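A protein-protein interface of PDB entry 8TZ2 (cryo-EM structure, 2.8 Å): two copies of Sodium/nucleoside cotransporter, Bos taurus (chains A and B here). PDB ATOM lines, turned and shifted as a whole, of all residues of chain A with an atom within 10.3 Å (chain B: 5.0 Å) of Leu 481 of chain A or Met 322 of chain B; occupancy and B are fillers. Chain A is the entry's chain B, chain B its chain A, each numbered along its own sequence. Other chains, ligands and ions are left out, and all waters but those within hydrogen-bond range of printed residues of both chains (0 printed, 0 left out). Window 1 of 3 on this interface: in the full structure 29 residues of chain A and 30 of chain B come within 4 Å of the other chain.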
ATOM      1  N   VAL A 473      20.822   8.882  -6.652  1.00  0.00           N
ATOM      2  CA  VAL A 473      19.689   8.507  -7.492  1.00  0.00           C
ATOM      3  C   VAL A 473      18.972   7.287  -6.918  1.00  0.00           C
ATOM      4  O   VAL A 473      17.734   7.221  -6.914  1.00  0.00           O
ATOM      5  CB  VAL A 473      20.168   8.273  -8.936  1.00  0.00           C
ATOM      6  CG1 VAL A 473      19.038   7.873  -9.824  1.00  0.00           C
ATOM      7  CG2 VAL A 473      20.787   9.534  -9.494  1.00  0.00           C
ATOM      8  N   ASN A 474      19.731   6.304  -6.433  1.00  0.00           N
ATOM      9  CA  ASN A 474      19.122   5.123  -5.840  1.00  0.00           C
ATOM     10  C   ASN A 474      18.298   5.488  -4.617  1.00  0.00           C
ATOM     11  O   ASN A 474      17.198   4.960  -4.424  1.00  0.00           O
ATOM     12  CB  ASN A 474      20.206   4.111  -5.481  1.00  0.00           C
ATOM     13  CG  ASN A 474      20.673   3.318  -6.676  1.00  0.00           C
ATOM     14  OD1 ASN A 474      20.473   3.720  -7.820  1.00  0.00           O
ATOM     15  ND2 ASN A 474      21.299   2.182  -6.418  1.00  0.00           N
ATOM     16  N   LEU A 475      18.807   6.389  -3.775  1.00  0.00           N
ATOM     17  CA  LEU A 475      18.029   6.802  -2.615  1.00  0.00           C
ATOM     18  C   LEU A 475      16.741   7.496  -3.035  1.00  0.00           C
ATOM     19  O   LEU A 475      15.669   7.213  -2.482  1.00  0.00           O
ATOM     20  CB  LEU A 475      18.867   7.716  -1.728  1.00  0.00           C
ATOM     21  CG  LEU A 475      19.743   7.017  -0.696  1.00  0.00           C
ATOM     22  CD1 LEU A 475      20.766   7.970  -0.121  1.00  0.00           C
ATOM     23  CD2 LEU A 475      18.861   6.475   0.397  1.00  0.00           C
ATOM     24  N   ILE A 476      16.819   8.387  -4.026  1.00  0.00           N
ATOM     25  CA  ILE A 476      15.610   9.069  -4.481  1.00  0.00           C
ATOM     26  C   ILE A 476      14.570   8.050  -4.929  1.00  0.00           C
ATOM     27  O   ILE A 476      13.411   8.074  -4.484  1.00  0.00           O
ATOM     28  CB  ILE A 476      15.949  10.051  -5.620  1.00  0.00           C
ATOM     29  CG1 ILE A 476      16.690  11.279  -5.100  1.00  0.00           C
ATOM     30  CG2 ILE A 476      14.702  10.459  -6.356  1.00  0.00           C
ATOM     31  CD1 ILE A 476      17.409  12.033  -6.180  1.00  0.00           C
ATOM     32  N   ALA A 477      14.981   7.120  -5.792  1.00  0.00           N
ATOM     33  CA  ALA A 477      14.041   6.161  -6.357  1.00  0.00           C
ATOM     34  C   ALA A 477      13.454   5.262  -5.278  1.00  0.00           C
ATOM     35  O   ALA A 477      12.242   5.021  -5.246  1.00  0.00           O
ATOM     36  CB  ALA A 477      14.740   5.334  -7.433  1.00  0.00           C
ATOM     37  N   PHE A 478      14.302   4.758  -4.378  1.00  0.00           N
ATOM     38  CA  PHE A 478      13.829   3.844  -3.349  1.00  0.00           C
ATOM     39  C   PHE A 478      12.843   4.528  -2.413  1.00  0.00           C
ATOM     40  O   PHE A 478      11.822   3.939  -2.046  1.00  0.00           O
ATOM     41  CB  PHE A 478      15.014   3.275  -2.563  1.00  0.00           C
ATOM     42  CG  PHE A 478      15.750   2.152  -3.264  1.00  0.00           C
ATOM     43  CD1 PHE A 478      15.115   1.327  -4.180  1.00  0.00           C
ATOM     44  CD2 PHE A 478      17.085   1.916  -2.989  1.00  0.00           C
ATOM     45  CE1 PHE A 478      15.795   0.306  -4.806  1.00  0.00           C
ATOM     46  CE2 PHE A 478      17.769   0.892  -3.615  1.00  0.00           C
ATOM     47  CZ  PHE A 478      17.122   0.090  -4.524  1.00  0.00           C
ATOM     48  N   LEU A 479      13.117   5.774  -2.019  1.00  0.00           N
ATOM     49  CA  LEU A 479      12.205   6.429  -1.090  1.00  0.00           C
ATOM     50  C   LEU A 479      10.892   6.814  -1.764  1.00  0.00           C
ATOM     51  O   LEU A 479       9.826   6.727  -1.134  1.00  0.00           O
ATOM     52  CB  LEU A 479      12.887   7.643  -0.469  1.00  0.00           C
ATOM     53  CG  LEU A 479      14.100   7.302   0.390  1.00  0.00           C
ATOM     54  CD1 LEU A 479      14.849   8.548   0.774  1.00  0.00           C
ATOM     55  CD2 LEU A 479      13.664   6.558   1.621  1.00  0.00           C
ATOM     56  N   ALA A 480      10.925   7.179  -3.049  1.00  0.00           N
ATOM     57  CA  ALA A 480       9.668   7.427  -3.747  1.00  0.00           C
ATOM     58  C   ALA A 480       8.847   6.148  -3.878  1.00  0.00           C
ATOM     59  O   ALA A 480       7.621   6.163  -3.697  1.00  0.00           O
ATOM     60  CB  ALA A 480       9.945   8.034  -5.118  1.00  0.00           C
ATOM     61  N   LEU A 481       9.509   5.028  -4.174  1.00  0.00           N
ATOM     62  CA  LEU A 481       8.807   3.753  -4.239  1.00  0.00           C
ATOM     63  C   LEU A 481       8.214   3.388  -2.890  1.00  0.00           C
ATOM     64  O   LEU A 481       7.107   2.845  -2.817  1.00  0.00           O
ATOM     65  CB  LEU A 481       9.750   2.651  -4.710  1.00  0.00           C
ATOM     66  CG  LEU A 481      10.152   2.633  -6.181  1.00  0.00           C
ATOM     67  CD1 LEU A 481      11.264   1.634  -6.376  1.00  0.00           C
ATOM     68  CD2 LEU A 481       8.972   2.296  -7.065  1.00  0.00           C
ATOM     69  N   LEU A 482       8.948   3.645  -1.809  1.00  0.00           N
ATOM     70  CA  LEU A 482       8.426   3.367  -0.478  1.00  0.00           C
ATOM     71  C   LEU A 482       7.164   4.173  -0.207  1.00  0.00           C
ATOM     72  O   LEU A 482       6.174   3.637   0.306  1.00  0.00           O
ATOM     73  CB  LEU A 482       9.497   3.672   0.565  1.00  0.00           C
ATOM     74  CG  LEU A 482       9.147   3.414   2.026  1.00  0.00           C
ATOM     75  CD1 LEU A 482       8.797   1.965   2.236  1.00  0.00           C
ATOM     76  CD2 LEU A 482      10.303   3.819   2.915  1.00  0.00           C
ATOM     77  N   SER A 483       7.173   5.460  -0.557  1.00  0.00           N
ATOM     78  CA  SER A 483       5.977   6.272  -0.356  1.00  0.00           C
ATOM     79  C   SER A 483       4.803   5.734  -1.164  1.00  0.00           C
ATOM     80  O   SER A 483       3.680   5.620  -0.651  1.00  0.00           O
ATOM     81  CB  SER A 483       6.263   7.721  -0.733  1.00  0.00           C
ATOM     82  OG  SER A 483       6.760   7.790  -2.051  1.00  0.00           O
ATOM     83  N   PHE A 484       5.046   5.375  -2.426  1.00  0.00           N
ATOM     84  CA  PHE A 484       3.961   4.865  -3.261  1.00  0.00           C
ATOM     85  C   PHE A 484       3.408   3.559  -2.710  1.00  0.00           C
ATOM     86  O   PHE A 484       2.187   3.364  -2.663  1.00  0.00           O
ATOM     87  CB  PHE A 484       4.448   4.683  -4.695  1.00  0.00           C
ATOM     88  CG  PHE A 484       3.541   3.847  -5.534  1.00  0.00           C
ATOM     89  CD1 PHE A 484       2.250   4.259  -5.798  1.00  0.00           C
ATOM     90  CD2 PHE A 484       3.979   2.650  -6.066  1.00  0.00           C
ATOM     91  CE1 PHE A 484       1.411   3.492  -6.570  1.00  0.00           C
ATOM     92  CE2 PHE A 484       3.143   1.880  -6.840  1.00  0.00           C
ATOM     93  CZ  PHE A 484       1.858   2.302  -7.092  1.00  0.00           C
ATOM     94  N   MET A 485       4.292   2.655  -2.287  1.00  0.00           N
ATOM     95  CA  MET A 485       3.857   1.374  -1.749  1.00  0.00           C
ATOM     96  C   MET A 485       3.042   1.556  -0.476  1.00  0.00           C
ATOM     97  O   MET A 485       2.021   0.888  -0.284  1.00  0.00           O
ATOM     98  CB  MET A 485       5.078   0.495  -1.495  1.00  0.00           C
ATOM     99  CG  MET A 485       4.760  -0.828  -0.845  1.00  0.00           C
ATOM    100  SD  MET A 485       6.057  -2.046  -1.108  1.00  0.00           S
ATOM    101  CE  MET A 485       7.477  -1.095  -0.594  1.00  0.00           C
ATOM    102  N   ASN A 486       3.474   2.463   0.405  1.00  0.00           N
ATOM    103  CA  ASN A 486       2.716   2.701   1.627  1.00  0.00           C
ATOM    104  C   ASN A 486       1.345   3.292   1.322  1.00  0.00           C
ATOM    105  O   ASN A 486       0.345   2.900   1.937  1.00  0.00           O
ATOM    106  CB  ASN A 486       3.505   3.611   2.564  1.00  0.00           C
ATOM    107  CG  ASN A 486       4.566   2.862   3.342  1.00  0.00           C
ATOM    108  OD1 ASN A 486       4.481   1.648   3.514  1.00  0.00           O
ATOM    109  ND2 ASN A 486       5.568   3.585   3.825  1.00  0.00           N
ATOM    110  N   SER A 487       1.268   4.219   0.364  1.00  0.00           N
ATOM    111  CA  SER A 487      -0.032   4.777   0.001  1.00  0.00           C
ATOM    112  C   SER A 487      -0.949   3.705  -0.572  1.00  0.00           C
ATOM    113  O   SER A 487      -2.134   3.640  -0.223  1.00  0.00           O
ATOM    114  CB  SER A 487       0.150   5.913  -1.000  1.00  0.00           C
ATOM    115  OG  SER A 487       0.688   5.426  -2.214  1.00  0.00           O
ATOM    116  N   ALA A 488      -0.414   2.846  -1.440  1.00  0.00           N
ATOM    117  CA  ALA A 488      -1.220   1.777  -2.017  1.00  0.00           C
ATOM    118  C   ALA A 488      -1.713   0.809  -0.949  1.00  0.00           C
ATOM    119  O   ALA A 488      -2.869   0.376  -0.981  1.00  0.00           O
ATOM    120  CB  ALA A 488      -0.408   1.034  -3.072  1.00  0.00           C
ATOM    121  N   LEU A 489      -0.847   0.452   0.001  1.00  0.00           N
ATOM    122  CA  LEU A 489      -1.251  -0.486   1.043  1.00  0.00           C
ATOM    123  C   LEU A 489      -2.285   0.122   1.980  1.00  0.00           C
ATOM    124  O   LEU A 489      -3.186  -0.583   2.443  1.00  0.00           O
ATOM    125  CB  LEU A 489      -0.027  -0.951   1.826  1.00  0.00           C
ATOM    126  CG  LEU A 489       0.909  -1.904   1.087  1.00  0.00           C
ATOM    127  CD1 LEU A 489       2.224  -2.031   1.812  1.00  0.00           C
ATOM    128  CD2 LEU A 489       0.266  -3.259   0.949  1.00  0.00           C
ATOM    129  N   SER A 502       1.008  -1.083   6.201  1.00  0.00           N
ATOM    130  CA  SER A 502       2.183  -0.463   5.614  1.00  0.00           C
ATOM    131  C   SER A 502       3.267  -1.509   5.413  1.00  0.00           C
ATOM    132  O   SER A 502       3.179  -2.636   5.906  1.00  0.00           O
ATOM    133  CB  SER A 502       2.699   0.682   6.487  1.00  0.00           C
ATOM    134  OG  SER A 502       3.109   0.212   7.757  1.00  0.00           O
ATOM    135  N   PHE A 503       4.297  -1.110   4.668  1.00  0.00           N
ATOM    136  CA  PHE A 503       5.480  -1.946   4.508  1.00  0.00           C
ATOM    137  C   PHE A 503       6.139  -2.224   5.856  1.00  0.00           C
ATOM    138  O   PHE A 503       6.562  -3.354   6.134  1.00  0.00           O
ATOM    139  CB  PHE A 503       6.448  -1.248   3.554  1.00  0.00           C
ATOM    140  CG  PHE A 503       7.785  -1.904   3.441  1.00  0.00           C
ATOM    141  CD1 PHE A 503       7.974  -2.976   2.595  1.00  0.00           C
ATOM    142  CD2 PHE A 503       8.862  -1.424   4.157  1.00  0.00           C
ATOM    143  CE1 PHE A 503       9.207  -3.569   2.482  1.00  0.00           C
ATOM    144  CE2 PHE A 503      10.092  -2.010   4.048  1.00  0.00           C
ATOM    145  CZ  PHE A 503      10.269  -3.082   3.206  1.00  0.00           C
ATOM    146  N   GLU A 504       6.210  -1.204   6.714  1.00  0.00           N
ATOM    147  CA  GLU A 504       6.821  -1.379   8.025  1.00  0.00           C
ATOM    148  C   GLU A 504       6.048  -2.385   8.866  1.00  0.00           C
ATOM    149  O   GLU A 504       6.648  -3.220   9.548  1.00  0.00           O
ATOM    150  CB  GLU A 504       6.905  -0.037   8.750  1.00  0.00           C
ATOM    151  CG  GLU A 504       7.883   0.956   8.139  1.00  0.00           C
ATOM    152  CD  GLU A 504       7.306   1.718   6.963  1.00  0.00           C
ATOM    153  OE1 GLU A 504       6.070   1.865   6.892  1.00  0.00           O
ATOM    154  OE2 GLU A 504       8.091   2.174   6.108  1.00  0.00           O
ATOM    155  N   TYR A 534      14.102  -2.929   5.561  1.00  0.00           N
ATOM    156  CA  TYR A 534      14.684  -1.829   4.803  1.00  0.00           C
ATOM    157  C   TYR A 534      15.987  -2.250   4.142  1.00  0.00           C
ATOM    158  O   TYR A 534      16.205  -1.977   2.956  1.00  0.00           O
ATOM    159  CB  TYR A 534      14.942  -0.632   5.717  1.00  0.00           C
ATOM    160  CG  TYR A 534      13.719   0.139   6.150  1.00  0.00           C
ATOM    161  CD1 TYR A 534      12.790   0.590   5.228  1.00  0.00           C
ATOM    162  CD2 TYR A 534      13.506   0.433   7.485  1.00  0.00           C
ATOM    163  CE1 TYR A 534      11.679   1.298   5.628  1.00  0.00           C
ATOM    164  CE2 TYR A 534      12.400   1.140   7.894  1.00  0.00           C
ATOM    165  CZ  TYR A 534      11.488   1.570   6.961  1.00  0.00           C
ATOM    166  OH  TYR A 534      10.381   2.276   7.360  1.00  0.00           O
ATOM    167  N   PHE A 537      15.355  -5.019   1.241  1.00  0.00           N
ATOM    168  CA  PHE A 537      14.626  -4.669   0.030  1.00  0.00           C
ATOM    169  C   PHE A 537      15.170  -3.443  -0.685  1.00  0.00           C
ATOM    170  O   PHE A 537      15.058  -3.368  -1.913  1.00  0.00           O
ATOM    171  CB  PHE A 537      13.149  -4.456   0.354  1.00  0.00           C
ATOM    172  CG  PHE A 537      12.419  -5.726   0.653  1.00  0.00           C
ATOM    173  CD1 PHE A 537      12.217  -6.664  -0.339  1.00  0.00           C
ATOM    174  CD2 PHE A 537      11.944  -5.990   1.923  1.00  0.00           C
ATOM    175  CE1 PHE A 537      11.557  -7.837  -0.075  1.00  0.00           C
ATOM    176  CE2 PHE A 537      11.280  -7.164   2.192  1.00  0.00           C
ATOM    177  CZ  PHE A 537      11.086  -8.089   1.192  1.00  0.00           C
ATOM    178  N   PHE A 538      15.752  -2.478   0.028  1.00  0.00           N
ATOM    179  CA  PHE A 538      16.290  -1.290  -0.633  1.00  0.00           C
ATOM    180  C   PHE A 538      17.801  -1.205  -0.515  1.00  0.00           C
ATOM    181  O   PHE A 538      18.491  -1.314  -1.532  1.00  0.00           O
ATOM    182  CB  PHE A 538      15.616  -0.048  -0.053  1.00  0.00           C
ATOM    183  CG  PHE A 538      14.117  -0.084  -0.119  1.00  0.00           C
ATOM    184  CD1 PHE A 538      13.461   0.028  -1.330  1.00  0.00           C
ATOM    185  CD2 PHE A 538      13.363  -0.230   1.028  1.00  0.00           C
ATOM    186  CE1 PHE A 538      12.089  -0.008  -1.392  1.00  0.00           C
ATOM    187  CE2 PHE A 538      11.990  -0.266   0.968  1.00  0.00           C
ATOM    188  CZ  PHE A 538      11.352  -0.155  -0.242  1.00  0.00           C
ATOM    189  N   VAL A 542      19.321   3.391   3.744  1.00  0.00           N
ATOM    190  CA  VAL A 542      17.986   3.658   4.269  1.00  0.00           C
ATOM    191  C   VAL A 542      17.866   3.133   5.695  1.00  0.00           C
ATOM    192  O   VAL A 542      17.361   3.818   6.600  1.00  0.00           O
ATOM    193  CB  VAL A 542      16.942   3.017   3.334  1.00  0.00           C
ATOM    194  CG1 VAL A 542      15.544   3.192   3.866  1.00  0.00           C
ATOM    195  CG2 VAL A 542      17.067   3.579   1.916  1.00  0.00           C
ATOM    196  N   PHE B 315      12.247   9.027 -11.054  1.00  0.00           N
ATOM    197  CA  PHE B 315      11.229   8.104 -10.572  1.00  0.00           C
ATOM    198  C   PHE B 315      10.458   7.479 -11.726  1.00  0.00           C
ATOM    199  O   PHE B 315      10.175   6.273 -11.720  1.00  0.00           O
ATOM    200  CB  PHE B 315      10.295   8.854  -9.627  1.00  0.00           C
ATOM    201  CG  PHE B 315       9.220   8.007  -9.030  1.00  0.00           C
ATOM    202  CD1 PHE B 315       9.508   6.769  -8.493  1.00  0.00           C
ATOM    203  CD2 PHE B 315       7.920   8.463  -8.985  1.00  0.00           C
ATOM    204  CE1 PHE B 315       8.517   5.999  -7.941  1.00  0.00           C
ATOM    205  CE2 PHE B 315       6.930   7.699  -8.433  1.00  0.00           C
ATOM    206  CZ  PHE B 315       7.225   6.467  -7.910  1.00  0.00           C
ATOM    207  N   THR B 318      12.544   4.873 -13.404  1.00  0.00           N
ATOM    208  CA  THR B 318      12.559   3.671 -12.576  1.00  0.00           C
ATOM    209  C   THR B 318      11.289   2.849 -12.774  1.00  0.00           C
ATOM    210  O   THR B 318      11.348   1.627 -12.972  1.00  0.00           O
ATOM    211  CB  THR B 318      12.719   4.062 -11.107  1.00  0.00           C
ATOM    212  OG1 THR B 318      13.949   4.771 -10.927  1.00  0.00           O
ATOM    213  CG2 THR B 318      12.720   2.850 -10.234  1.00  0.00           C
ATOM    214  N   VAL B 319      10.130   3.508 -12.743  1.00  0.00           N
ATOM    215  CA  VAL B 319       8.869   2.786 -12.872  1.00  0.00           C
ATOM    216  C   VAL B 319       8.749   2.156 -14.254  1.00  0.00           C
ATOM    217  O   VAL B 319       8.248   1.033 -14.394  1.00  0.00           O
ATOM    218  CB  VAL B 319       7.685   3.719 -12.571  1.00  0.00           C
ATOM    219  CG1 VAL B 319       6.380   3.005 -12.836  1.00  0.00           C
ATOM    220  CG2 VAL B 319       7.740   4.194 -11.143  1.00  0.00           C
ATOM    221  N   MET B 320       9.183   2.867 -15.296  1.00  0.00           N
ATOM    222  CA  MET B 320       9.113   2.306 -16.640  1.00  0.00           C
ATOM    223  C   MET B 320      10.006   1.080 -16.770  1.00  0.00           C
ATOM    224  O   MET B 320       9.635   0.102 -17.426  1.00  0.00           O
ATOM    225  CB  MET B 320       9.493   3.363 -17.674  1.00  0.00           C
ATOM    226  CG  MET B 320       8.509   4.516 -17.777  1.00  0.00           C
ATOM    227  SD  MET B 320       6.862   4.022 -18.310  1.00  0.00           S
ATOM    228  CE  MET B 320       7.213   3.460 -19.970  1.00  0.00           C
ATOM    229  N   SER B 321      11.190   1.110 -16.152  1.00  0.00           N
ATOM    230  CA  SER B 321      12.051  -0.069 -16.181  1.00  0.00           C
ATOM    231  C   SER B 321      11.400  -1.240 -15.455  1.00  0.00           C
ATOM    232  O   SER B 321      11.456  -2.385 -15.925  1.00  0.00           O
ATOM    233  CB  SER B 321      13.411   0.259 -15.573  1.00  0.00           C
ATOM    234  OG  SER B 321      13.309   0.496 -14.184  1.00  0.00           O
ATOM    235  N   MET B 322      10.758  -0.972 -14.318  1.00  0.00           N
ATOM    236  CA  MET B 322      10.070  -2.044 -13.603  1.00  0.00           C
ATOM    237  C   MET B 322       8.958  -2.643 -14.458  1.00  0.00           C
ATOM    238  O   MET B 322       8.813  -3.871 -14.538  1.00  0.00           O
ATOM    239  CB  MET B 322       9.508  -1.511 -12.288  1.00  0.00           C
ATOM    240  CG  MET B 322      10.549  -0.923 -11.350  1.00  0.00           C
ATOM    241  SD  MET B 322       9.829   0.007  -9.992  1.00  0.00           S
ATOM    242  CE  MET B 322       9.349  -1.332  -8.922  1.00  0.00           C
ATOM    243  N   LEU B 323       8.170  -1.790 -15.112  1.00  0.00           N
ATOM    244  CA  LEU B 323       7.079  -2.276 -15.952  1.00  0.00           C
ATOM    245  C   LEU B 323       7.604  -3.071 -17.140  1.00  0.00           C
ATOM    246  O   LEU B 323       6.999  -4.073 -17.536  1.00  0.00           O
ATOM    247  CB  LEU B 323       6.224  -1.106 -16.437  1.00  0.00           C
ATOM    248  CG  LEU B 323       5.435  -0.309 -15.399  1.00  0.00           C
ATOM    249  CD1 LEU B 323       4.791   0.875 -16.066  1.00  0.00           C
ATOM    250  CD2 LEU B 323       4.385  -1.160 -14.728  1.00  0.00           C
ATOM    251  N   TYR B 324       8.718  -2.635 -17.730  1.00  0.00           N
ATOM    252  CA  TYR B 324       9.318  -3.401 -18.816  1.00  0.00           C
ATOM    253  C   TYR B 324       9.769  -4.769 -18.330  1.00  0.00           C
ATOM    254  O   TYR B 324       9.648  -5.763 -19.053  1.00  0.00           O
ATOM    255  CB  TYR B 324      10.488  -2.633 -19.425  1.00  0.00           C
ATOM    256  CG  TYR B 324      10.915  -3.164 -20.767  1.00  0.00           C
ATOM    257  CD1 TYR B 324      10.219  -2.828 -21.914  1.00  0.00           C
ATOM    258  CD2 TYR B 324      12.010  -4.005 -20.889  1.00  0.00           C
ATOM    259  CE1 TYR B 324      10.595  -3.313 -23.143  1.00  0.00           C
ATOM    260  CE2 TYR B 324      12.397  -4.496 -22.116  1.00  0.00           C
ATOM    261  CZ  TYR B 324      11.687  -4.145 -23.242  1.00  0.00           C
ATOM    262  OH  TYR B 324      12.064  -4.633 -24.470  1.00  0.00           O
ATOM    263  N   TYR B 325      10.305  -4.841 -17.110  1.00  0.00           N
ATOM    264  CA  TYR B 325      10.643  -6.145 -16.550  1.00  0.00           C
ATOM    265  C   TYR B 325       9.405  -7.020 -16.401  1.00  0.00           C
ATOM    266  O   TYR B 325       9.430  -8.207 -16.752  1.00  0.00           O
ATOM    267  CB  TYR B 325      11.339  -5.986 -15.201  1.00  0.00           C
ATOM    268  CG  TYR B 325      11.441  -7.276 -14.429  1.00  0.00           C
ATOM    269  CD1 TYR B 325      12.433  -8.197 -14.714  1.00  0.00           C
ATOM    270  CD2 TYR B 325      10.539  -7.577 -13.421  1.00  0.00           C
ATOM    271  CE1 TYR B 325      12.528  -9.377 -14.019  1.00  0.00           C
ATOM    272  CE2 TYR B 325      10.626  -8.758 -12.719  1.00  0.00           C
ATOM    273  CZ  TYR B 325      11.623  -9.654 -13.022  1.00  0.00           C
ATOM    274  OH  TYR B 325      11.723 -10.836 -12.330  1.00  0.00           O
ATOM    275  N   LEU B 326       8.309  -6.457 -15.891  1.00  0.00           N
ATOM    276  CA  LEU B 326       7.117  -7.264 -15.649  1.00  0.00           C
ATOM    277  C   LEU B 326       6.419  -7.687 -16.935  1.00  0.00           C
ATOM    278  O   LEU B 326       5.635  -8.641 -16.909  1.00  0.00           O
ATOM    279  CB  LEU B 326       6.127  -6.506 -14.766  1.00  0.00           C
ATOM    280  CG  LEU B 326       6.536  -6.207 -13.326  1.00  0.00           C
ATOM    281  CD1 LEU B 326       5.563  -5.228 -12.711  1.00  0.00           C
ATOM    282  CD2 LEU B 326       6.592  -7.469 -12.502  1.00  0.00           C
ATOM    283  N   LEU B 453      12.799  -7.616  -9.685  1.00  0.00           N
ATOM    284  CA  LEU B 453      12.170  -6.309  -9.829  1.00  0.00           C
ATOM    285  C   LEU B 453      13.047  -5.194  -9.276  1.00  0.00           C
ATOM    286  O   LEU B 453      13.122  -4.103  -9.856  1.00  0.00           O
ATOM    287  CB  LEU B 453      10.821  -6.332  -9.118  1.00  0.00           C
ATOM    288  CG  LEU B 453       9.858  -5.168  -9.303  1.00  0.00           C
ATOM    289  CD1 LEU B 453       9.474  -4.988 -10.755  1.00  0.00           C
ATOM    290  CD2 LEU B 453       8.641  -5.432  -8.459  1.00  0.00           C
ATOM    291  N   ALA B 456      15.749  -4.257 -11.577  1.00  0.00           N
ATOM    292  CA  ALA B 456      15.198  -3.411 -12.624  1.00  0.00           C
ATOM    293  C   ALA B 456      15.036  -1.979 -12.139  1.00  0.00           C
ATOM    294  O   ALA B 456      15.298  -1.032 -12.887  1.00  0.00           O
ATOM    295  CB  ALA B 456      13.862  -3.978 -13.098  1.00  0.00           C
ATOM    296  N   ALA B 457      14.610  -1.800 -10.886  1.00  0.00           N
ATOM    297  CA  ALA B 457      14.497  -0.455 -10.336  1.00  0.00           C
ATOM    298  C   ALA B 457      15.854   0.239 -10.280  1.00  0.00           C
ATOM    299  O   ALA B 457      15.976   1.413 -10.650  1.00  0.00           O
ATOM    300  CB  ALA B 457      13.858  -0.518  -8.951  1.00  0.00           C
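OG of Ser 321 of chain B sits at hydrogen-bond distance from O of Thr 318 of chain B, at 2.6 Å. O of Ala 480 of chain A lies within hydrogen-bond range of OG of Ser 483 of chain A (2.5 Å).
Among the printed residues, pairs that only touch across the chains: Ala 477 of chain A with Thr 318 of chain B (3.6 Å), Ala 480 of chain A with Phe 315 of chain B (3.6 Å), Leu 481 of chain A with Phe 315 of chain B (3.8 Å) and Leu 481 of chain A with Met 322 of chain B (3.8 Å).
Val 473 of chain A touches none of the printed residues of chain B. Of the printed residues of chain B, Ala 477 of chain A touches Thr 318. Leu 481 of chain A touches just these residues of chain B: Phe 315 and Met 322. Printed residues of chain A within 4 Å of Phe 315 of chain B: Ala 480 (3.6 Å) and Leu 481 (3.8 Å). Thr 318 of chain B touches one residue of chain A. No residue of chain A comes within 4 Å of Ser 321 of chain B. Printed residues of chain A within 4 Å of Met 322 of chain B: Leu 481 (3.8 Å). No residue of chain A comes within 4 Å of Leu 326 of chain B. No residue of chain A comes within 4 Å of Ala 457 of chain B.
Printed residues of chain B that touch a printed residue of chain A: Phe 315, Thr 318 and Met 322. Hydrophobic or aromatic side chains of chain B that line the printed part of chain A: Phe 315 and Met 322. Printed residues of chain A that touch a printed residue of chain B: Ala 477, Ala 480 and Leu 481. Among the printed residues, 4 pairs touch across the chains.
No position is printed for both chains.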
